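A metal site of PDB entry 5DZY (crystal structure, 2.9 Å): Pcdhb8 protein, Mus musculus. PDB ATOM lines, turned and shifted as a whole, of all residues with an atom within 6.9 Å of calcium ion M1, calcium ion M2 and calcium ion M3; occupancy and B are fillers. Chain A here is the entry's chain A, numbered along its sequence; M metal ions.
The side-chain carboxylate (OE1) of Glu 225 sits close to the backbone NH (N) of Phe 280.
The backbone carbonyl oxygen (O) of Leu 309 lies within hydrogen-bond range of the backbone NH (N) of Glu 225, 3.1 Å away.
The side-chain carboxylate (OD1) of Asp 313 sits close to the side-chain amide oxygen (OD1) of Asn 314 (3.5 Å).
The side-chain carboxylate (OD2) of Asp 310 lies within hydrogen-bond range of the side-chain amide nitrogen (ND2) of Asn 349.
N of Ala 282 sits at hydrogen-bond distance from OD2 of Asp 279, 2.8 Å away.
The side-chain carboxylate (OD2) of Asp 310 lies within hydrogen-bond range of the side-chain hydroxyl (OG) of Ser 346 (3.0 Å).
The backbone NH (N) of Leu 402 lies within hydrogen-bond range of the side-chain carboxylate (OD1) of Asp 396 (2.6 Å).
The nearest printed residue that does not touch calcium ion M1 is Phe 280 (4.8 Å).
Six residues have an atom within 4 Å of calcium ion M3: Asn 312, Asn 314, Asp 343, Asp 345, Asn 349 and Asp 396.
The side-chain carboxylate (OE2) of Glu 225 is bound to calcium ion M1 (2.2 Å).
Calcium ion M1 is bound by the side-chain carboxylate (OD2) of Asp 313 (2.4 Å).
OE1 of Glu 281 binds calcium ion M1, at 2.5 Å.
OD1 of Asp 279 binds calcium ion M1, at 2.5 Å.
Calcium ion M1 is bound by the side-chain carboxylate (OD1) of Asp 313 (2.7 Å).
Calcium ion M1 has five donor atoms within binding distance.
Calcium ion M2 is bound by the side-chain carboxylate (OE2) of Glu 281 (2.2 Å), the backbone carbonyl oxygen (O) of Val 311 (2.5 Å), the side-chain carboxylate (OD1) of Asp 313 (2.6 Å), the side-chain carboxylate (OD1) of Asp 310 (2.7 Å), the side-chain carboxylate (OE1) of Glu 281 (2.7 Å) and the side-chain carboxylate (OD1) of Asp 345 (2.8 Å).
Slightly farther from calcium ion M2 lies OE1 of Glu 225 (3.1 Å).
Calcium ion M3 is bound by the side-chain carboxylate (OD2) of Asp 345 (2.5 Å), the backbone carbonyl oxygen (O) of Asn 349 (2.5 Å), the backbone carbonyl oxygen (O) of Asn 314 (2.6 Å), the side-chain amide oxygen (OD1) of Asn 312 (2.8 Å) and the side-chain carboxylate (OD2) of Asp 343 (2.8 Å).
Slightly farther from calcium ion M3 lies OD2 of Asp 396 (3.0 Å).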
ATOM      1  N   GLU A 225       6.428  14.619  -2.739  1.00  0.00           N
ATOM      2  CA  GLU A 225       7.099  13.634  -3.582  1.00  0.00           C
ATOM      3  C   GLU A 225       7.548  12.420  -2.772  1.00  0.00           C
ATOM      4  O   GLU A 225       7.517  11.289  -3.255  1.00  0.00           O
ATOM      5  CB  GLU A 225       8.294  14.259  -4.283  1.00  0.00           C
ATOM      6  CG  GLU A 225       9.106  13.299  -5.141  1.00  0.00           C
ATOM      7  CD  GLU A 225      10.307  13.960  -5.790  1.00  0.00           C
ATOM      8  OE1 GLU A 225      10.460  15.199  -5.639  1.00  0.00           O
ATOM      9  OE2 GLU A 225      11.088  13.255  -6.452  1.00  0.00           O
ATOM     10  N   LEU A 278       6.400   8.551  -6.799  1.00  0.00           N
ATOM     11  CA  LEU A 278       6.209   9.906  -7.297  1.00  0.00           C
ATOM     12  C   LEU A 278       7.541  10.646  -7.413  1.00  0.00           C
ATOM     13  O   LEU A 278       8.429  10.469  -6.586  1.00  0.00           O
ATOM     14  CB  LEU A 278       5.263  10.702  -6.392  1.00  0.00           C
ATOM     15  CG  LEU A 278       3.763  10.538  -6.659  1.00  0.00           C
ATOM     16  CD1 LEU A 278       2.959  11.414  -5.714  1.00  0.00           C
ATOM     17  CD2 LEU A 278       3.445  10.867  -8.108  1.00  0.00           C
ATOM     18  N   ASP A 279       7.664  11.449  -8.466  1.00  0.00           N
ATOM     19  CA  ASP A 279       8.874  12.255  -8.664  1.00  0.00           C
ATOM     20  C   ASP A 279       8.516  13.598  -9.285  1.00  0.00           C
ATOM     21  O   ASP A 279       8.029  13.665 -10.416  1.00  0.00           O
ATOM     22  CB  ASP A 279       9.876  11.511  -9.552  1.00  0.00           C
ATOM     23  CG  ASP A 279      11.217  12.203  -9.612  1.00  0.00           C
ATOM     24  OD1 ASP A 279      12.083  11.885  -8.775  1.00  0.00           O
ATOM     25  OD2 ASP A 279      11.410  13.063 -10.505  1.00  0.00           O
ATOM     26  N   PHE A 280       8.771  14.672  -8.533  1.00  0.00           N
ATOM     27  CA  PHE A 280       8.449  16.018  -8.975  1.00  0.00           C
ATOM     28  C   PHE A 280       9.224  16.414 -10.224  1.00  0.00           C
ATOM     29  O   PHE A 280       8.774  17.240 -11.014  1.00  0.00           O
ATOM     30  CB  PHE A 280       8.721  17.010  -7.842  1.00  0.00           C
ATOM     31  CG  PHE A 280       8.398  18.436  -8.184  1.00  0.00           C
ATOM     32  CD1 PHE A 280       7.108  18.921  -8.070  1.00  0.00           C
ATOM     33  CD2 PHE A 280       9.390  19.307  -8.621  1.00  0.00           C
ATOM     34  CE1 PHE A 280       6.805  20.233  -8.383  1.00  0.00           C
ATOM     35  CE2 PHE A 280       9.097  20.621  -8.937  1.00  0.00           C
ATOM     36  CZ  PHE A 280       7.805  21.084  -8.814  1.00  0.00           C
ATOM     37  N   GLU A 281      10.398  15.806 -10.401  1.00  0.00           N
ATOM     38  CA  GLU A 281      11.269  16.133 -11.518  1.00  0.00           C
ATOM     39  C   GLU A 281      10.826  15.422 -12.797  1.00  0.00           C
ATOM     40  O   GLU A 281      11.158  15.857 -13.902  1.00  0.00           O
ATOM     41  CB  GLU A 281      12.722  15.770 -11.193  1.00  0.00           C
ATOM     42  CG  GLU A 281      13.382  16.684 -10.178  1.00  0.00           C
ATOM     43  CD  GLU A 281      12.789  16.562  -8.795  1.00  0.00           C
ATOM     44  OE1 GLU A 281      12.448  15.427  -8.397  1.00  0.00           O
ATOM     45  OE2 GLU A 281      12.655  17.594  -8.103  1.00  0.00           O
ATOM     46  N   ALA A 282      10.084  14.331 -12.651  1.00  0.00           N
ATOM     47  CA  ALA A 282       9.556  13.612 -13.795  1.00  0.00           C
ATOM     48  C   ALA A 282       8.193  14.175 -14.202  1.00  0.00           C
ATOM     49  O   ALA A 282       8.034  14.681 -15.313  1.00  0.00           O
ATOM     50  CB  ALA A 282       9.438  12.127 -13.485  1.00  0.00           C
ATOM     51  N   LEU A 309       4.480  17.980  -4.659  1.00  0.00           N
ATOM     52  CA  LEU A 309       5.376  18.919  -3.999  1.00  0.00           C
ATOM     53  C   LEU A 309       6.828  18.495  -4.197  1.00  0.00           C
ATOM     54  O   LEU A 309       7.142  17.305  -4.208  1.00  0.00           O
ATOM     55  CB  LEU A 309       5.057  19.024  -2.516  1.00  0.00           C
ATOM     56  CG  LEU A 309       3.665  19.551  -2.142  1.00  0.00           C
ATOM     57  CD1 LEU A 309       3.498  19.575  -0.631  1.00  0.00           C
ATOM     58  CD2 LEU A 309       3.444  20.935  -2.743  1.00  0.00           C
ATOM     59  N   ASP A 310       7.716  19.478  -4.357  1.00  0.00           N
ATOM     60  CA  ASP A 310       9.129  19.203  -4.575  1.00  0.00           C
ATOM     61  C   ASP A 310       9.841  18.863  -3.263  1.00  0.00           C
ATOM     62  O   ASP A 310       9.638  19.519  -2.241  1.00  0.00           O
ATOM     63  CB  ASP A 310       9.814  20.387  -5.247  1.00  0.00           C
ATOM     64  CG  ASP A 310      11.300  20.152  -5.476  1.00  0.00           C
ATOM     65  OD1 ASP A 310      11.682  18.991  -5.722  1.00  0.00           O
ATOM     66  OD2 ASP A 310      12.075  21.128  -5.419  1.00  0.00           O
ATOM     67  N   VAL A 311      10.677  17.833  -3.306  1.00  0.00           N
ATOM     68  CA  VAL A 311      11.505  17.453  -2.174  1.00  0.00           C
ATOM     69  C   VAL A 311      12.971  17.408  -2.597  1.00  0.00           C
ATOM     70  O   VAL A 311      13.300  16.835  -3.625  1.00  0.00           O
ATOM     71  CB  VAL A 311      11.095  16.087  -1.587  1.00  0.00           C
ATOM     72  CG1 VAL A 311      11.951  15.734  -0.378  1.00  0.00           C
ATOM     73  CG2 VAL A 311       9.612  16.095  -1.213  1.00  0.00           C
ATOM     74  N   ASN A 312      13.842  18.020  -1.800  1.00  0.00           N
ATOM     75  CA  ASN A 312      15.264  18.031  -2.109  1.00  0.00           C
ATOM     76  C   ASN A 312      15.873  16.644  -1.991  1.00  0.00           C
ATOM     77  O   ASN A 312      16.480  16.299  -0.971  1.00  0.00           O
ATOM     78  CB  ASN A 312      16.000  19.010  -1.201  1.00  0.00           C
ATOM     79  CG  ASN A 312      17.435  19.250  -1.638  1.00  0.00           C
ATOM     80  OD1 ASN A 312      17.785  19.023  -2.800  1.00  0.00           O
ATOM     81  ND2 ASN A 312      18.263  19.731  -0.718  1.00  0.00           N
ATOM     82  N   ASP A 313      15.711  15.831  -3.034  1.00  0.00           N
ATOM     83  CA  ASP A 313      16.213  14.465  -3.026  1.00  0.00           C
ATOM     84  C   ASP A 313      17.232  14.236  -4.143  1.00  0.00           C
ATOM     85  O   ASP A 313      17.556  13.095  -4.483  1.00  0.00           O
ATOM     86  CB  ASP A 313      15.059  13.471  -3.155  1.00  0.00           C
ATOM     87  CG  ASP A 313      14.283  13.628  -4.457  1.00  0.00           C
ATOM     88  OD1 ASP A 313      14.381  14.707  -5.081  1.00  0.00           O
ATOM     89  OD2 ASP A 313      13.579  12.675  -4.845  1.00  0.00           O
ATOM     90  N   ASN A 314      17.732  15.331  -4.725  1.00  0.00           N
ATOM     91  CA  ASN A 314      18.733  15.244  -5.774  1.00  0.00           C
ATOM     92  C   ASN A 314      19.993  16.039  -5.460  1.00  0.00           C
ATOM     93  O   ASN A 314      19.923  17.232  -5.130  1.00  0.00           O
ATOM     94  CB  ASN A 314      18.150  15.712  -7.113  1.00  0.00           C
ATOM     95  CG  ASN A 314      17.266  14.670  -7.762  1.00  0.00           C
ATOM     96  OD1 ASN A 314      16.102  14.924  -8.066  1.00  0.00           O
ATOM     97  ND2 ASN A 314      17.816  13.484  -7.982  1.00  0.00           N
ATOM     98  N   ALA A 315      21.138  15.384  -5.566  1.00  0.00           N
ATOM     99  CA  ALA A 315      22.427  16.048  -5.376  1.00  0.00           C
ATOM    100  C   ALA A 315      22.872  16.705  -6.676  1.00  0.00           C
ATOM    101  O   ALA A 315      22.584  16.201  -7.763  1.00  0.00           O
ATOM    102  CB  ALA A 315      23.471  15.054  -4.886  1.00  0.00           C
ATOM    103  N   PRO A 316      23.570  17.853  -6.570  1.00  0.00           N
ATOM    104  CA  PRO A 316      24.083  18.561  -7.752  1.00  0.00           C
ATOM    105  C   PRO A 316      25.010  17.700  -8.602  1.00  0.00           C
ATOM    106  O   PRO A 316      25.859  16.994  -8.058  1.00  0.00           O
ATOM    107  CB  PRO A 316      24.846  19.746  -7.148  1.00  0.00           C
ATOM    108  CG  PRO A 316      24.222  19.955  -5.808  1.00  0.00           C
ATOM    109  CD  PRO A 316      23.845  18.581  -5.328  1.00  0.00           C
ATOM    110  N   SER A 342      24.677  20.857 -12.563  1.00  0.00           N
ATOM    111  CA  SER A 342      23.287  20.573 -12.896  1.00  0.00           C
ATOM    112  C   SER A 342      22.458  20.280 -11.653  1.00  0.00           C
ATOM    113  O   SER A 342      22.979  19.852 -10.630  1.00  0.00           O
ATOM    114  CB  SER A 342      23.200  19.407 -13.880  1.00  0.00           C
ATOM    115  OG  SER A 342      21.858  19.112 -14.209  1.00  0.00           O
ATOM    116  N   ASP A 343      21.150  20.510 -11.750  1.00  0.00           N
ATOM    117  CA  ASP A 343      20.223  20.226 -10.664  1.00  0.00           C
ATOM    118  C   ASP A 343      18.790  20.187 -11.180  1.00  0.00           C
ATOM    119  O   ASP A 343      18.252  21.208 -11.599  1.00  0.00           O
ATOM    120  CB  ASP A 343      20.356  21.270  -9.544  1.00  0.00           C
ATOM    121  CG  ASP A 343      19.776  20.798  -8.230  1.00  0.00           C
ATOM    122  OD1 ASP A 343      18.877  19.930  -8.238  1.00  0.00           O
ATOM    123  OD2 ASP A 343      20.217  21.302  -7.174  1.00  0.00           O
ATOM    124  N   PRO A 344      18.163  19.002 -11.132  1.00  0.00           N
ATOM    125  CA  PRO A 344      16.793  18.808 -11.625  1.00  0.00           C
ATOM    126  C   PRO A 344      15.743  19.398 -10.687  1.00  0.00           C
ATOM    127  O   PRO A 344      14.595  19.587 -11.096  1.00  0.00           O
ATOM    128  CB  PRO A 344      16.665  17.294 -11.706  1.00  0.00           C
ATOM    129  CG  PRO A 344      17.588  16.793 -10.656  1.00  0.00           C
ATOM    130  CD  PRO A 344      18.747  17.743 -10.647  1.00  0.00           C
ATOM    131  N   ASP A 345      16.124  19.674  -9.445  1.00  0.00           N
ATOM    132  CA  ASP A 345      15.200  20.225  -8.457  1.00  0.00           C
ATOM    133  C   ASP A 345      14.789  21.650  -8.801  1.00  0.00           C
ATOM    134  O   ASP A 345      15.326  22.264  -9.721  1.00  0.00           O
ATOM    135  CB  ASP A 345      15.823  20.183  -7.054  1.00  0.00           C
ATOM    136  CG  ASP A 345      16.144  18.773  -6.605  1.00  0.00           C
ATOM    137  OD1 ASP A 345      15.454  17.829  -7.039  1.00  0.00           O
ATOM    138  OD2 ASP A 345      17.095  18.605  -5.809  1.00  0.00           O
ATOM    139  N   SER A 346      13.816  22.172  -8.052  1.00  0.00           N
ATOM    140  CA  SER A 346      13.319  23.530  -8.285  1.00  0.00           C
ATOM    141  C   SER A 346      13.520  24.419  -7.060  1.00  0.00           C
ATOM    142  O   SER A 346      13.749  23.921  -5.962  1.00  0.00           O
ATOM    143  CB  SER A 346      11.842  23.491  -8.668  1.00  0.00           C
ATOM    144  OG  SER A 346      11.057  22.926  -7.628  1.00  0.00           O
ATOM    145  N   ASP A 348      15.163  26.850  -4.341  1.00  0.00           N
ATOM    146  CA  ASP A 348      16.485  26.846  -3.705  1.00  0.00           C
ATOM    147  C   ASP A 348      17.083  25.446  -3.732  1.00  0.00           C
ATOM    148  O   ASP A 348      18.297  25.281  -3.599  1.00  0.00           O
ATOM    149  CB  ASP A 348      16.383  27.353  -2.272  1.00  0.00           C
ATOM    150  CG  ASP A 348      15.981  28.813  -2.193  1.00  0.00           C
ATOM    151  OD1 ASP A 348      16.120  29.523  -3.214  1.00  0.00           O
ATOM    152  OD2 ASP A 348      15.529  29.257  -1.120  1.00  0.00           O
ATOM    153  N   ASN A 349      16.236  24.438  -3.905  1.00  0.00           N
ATOM    154  CA  ASN A 349      16.694  23.062  -4.041  1.00  0.00           C
ATOM    155  C   ASN A 349      17.426  22.877  -5.364  1.00  0.00           C
ATOM    156  O   ASN A 349      18.276  21.999  -5.499  1.00  0.00           O
ATOM    157  CB  ASN A 349      15.520  22.083  -3.951  1.00  0.00           C
ATOM    158  CG  ASN A 349      14.745  22.231  -2.658  1.00  0.00           C
ATOM    159  OD1 ASN A 349      15.283  22.628  -1.632  1.00  0.00           O
ATOM    160  ND2 ASN A 349      13.457  21.910  -2.711  1.00  0.00           N
ATOM    161  N   GLY A 350      17.095  23.717  -6.343  1.00  0.00           N
ATOM    162  CA  GLY A 350      17.727  23.681  -7.643  1.00  0.00           C
ATOM    163  C   GLY A 350      18.867  24.675  -7.753  1.00  0.00           C
ATOM    164  O   GLY A 350      19.808  24.471  -8.524  1.00  0.00           O
ATOM    165  N   ARG A 351      18.793  25.750  -6.973  1.00  0.00           N
ATOM    166  CA  ARG A 351      19.848  26.754  -6.935  1.00  0.00           C
ATOM    167  C   ARG A 351      21.077  26.190  -6.239  1.00  0.00           C
ATOM    168  O   ARG A 351      20.950  25.523  -5.208  1.00  0.00           O
ATOM    169  CB  ARG A 351      19.372  28.026  -6.248  1.00  0.00           C
ATOM    170  CG  ARG A 351      20.401  29.141  -6.227  1.00  0.00           C
ATOM    171  CD  ARG A 351      19.822  30.442  -5.694  1.00  0.00           C
ATOM    172  NE  ARG A 351      18.701  30.914  -6.508  1.00  0.00           N
ATOM    173  CZ  ARG A 351      17.471  31.084  -6.052  1.00  0.00           C
ATOM    174  NH1 ARG A 351      17.197  30.835  -4.776  1.00  0.00           N
ATOM    175  NH2 ARG A 351      16.505  31.519  -6.858  1.00  0.00           N
ATOM    176  N   ASP A 396      23.913  22.845  -3.024  1.00  0.00           N
ATOM    177  CA  ASP A 396      22.647  23.536  -3.223  1.00  0.00           C
ATOM    178  C   ASP A 396      22.284  24.420  -2.027  1.00  0.00           C
ATOM    179  O   ASP A 396      22.900  24.321  -0.963  1.00  0.00           O
ATOM    180  CB  ASP A 396      21.516  22.536  -3.489  1.00  0.00           C
ATOM    181  CG  ASP A 396      21.494  21.391  -2.492  1.00  0.00           C
ATOM    182  OD1 ASP A 396      21.915  21.585  -1.332  1.00  0.00           O
ATOM    183  OD2 ASP A 396      21.053  20.282  -2.874  1.00  0.00           O
ATOM    184  N   LEU A 397      21.287  25.266  -2.204  1.00  0.00           N
ATOM    185  CA  LEU A 397      20.836  26.157  -1.136  1.00  0.00           C
ATOM    186  C   LEU A 397      19.484  25.723  -0.580  1.00  0.00           C
ATOM    187  O   LEU A 397      18.717  26.547  -0.075  1.00  0.00           O
ATOM    188  CB  LEU A 397      20.745  27.600  -1.652  1.00  0.00           C
ATOM    189  CG  LEU A 397      22.061  28.249  -2.097  1.00  0.00           C
ATOM    190  CD1 LEU A 397      21.813  29.656  -2.624  1.00  0.00           C
ATOM    191  CD2 LEU A 397      23.062  28.262  -0.958  1.00  0.00           C
ATOM    192  N   GLY A 398      19.202  24.424  -0.679  1.00  0.00           N
ATOM    193  CA  GLY A 398      17.938  23.889  -0.213  1.00  0.00           C
ATOM    194  C   GLY A 398      17.994  23.385   1.220  1.00  0.00           C
ATOM    195  O   GLY A 398      19.034  23.467   1.873  1.00  0.00           O
ATOM    196  N   PRO A 400      16.913  19.911   3.445  1.00  0.00           N
ATOM    197  CA  PRO A 400      18.320  19.969   3.865  1.00  0.00           C
ATOM    198  C   PRO A 400      19.278  20.209   2.702  1.00  0.00           C
ATOM    199  O   PRO A 400      18.905  20.027   1.537  1.00  0.00           O
ATOM    200  CB  PRO A 400      18.569  18.580   4.478  1.00  0.00           C
ATOM    201  CG  PRO A 400      17.210  18.003   4.720  1.00  0.00           C
ATOM    202  CD  PRO A 400      16.347  18.555   3.631  1.00  0.00           C
ATOM    203  N   LEU A 402      22.367  19.570   0.221  1.00  0.00           N
ATOM    204  CA  LEU A 402      23.106  18.459  -0.356  1.00  0.00           C
ATOM    205  C   LEU A 402      24.392  18.946  -1.034  1.00  0.00           C
ATOM    206  O   LEU A 402      24.378  19.914  -1.796  1.00  0.00           O
ATOM    207  CB  LEU A 402      22.250  17.704  -1.368  1.00  0.00           C
ATOM    208  CG  LEU A 402      20.981  17.033  -0.834  1.00  0.00           C
ATOM    209  CD1 LEU A 402      20.223  16.348  -1.950  1.00  0.00           C
ATOM    210  CD2 LEU A 402      21.329  16.045   0.267  1.00  0.00           C
HETATM  211 CA    CA M   1      13.182  13.418  -7.142  1.00  0.00          CA
HETATM  212 CA    CA M   2      13.082  16.740  -6.077  1.00  0.00          CA
HETATM  213 CA    CA M   3      19.171  19.705  -5.100  1.00  0.00          CA
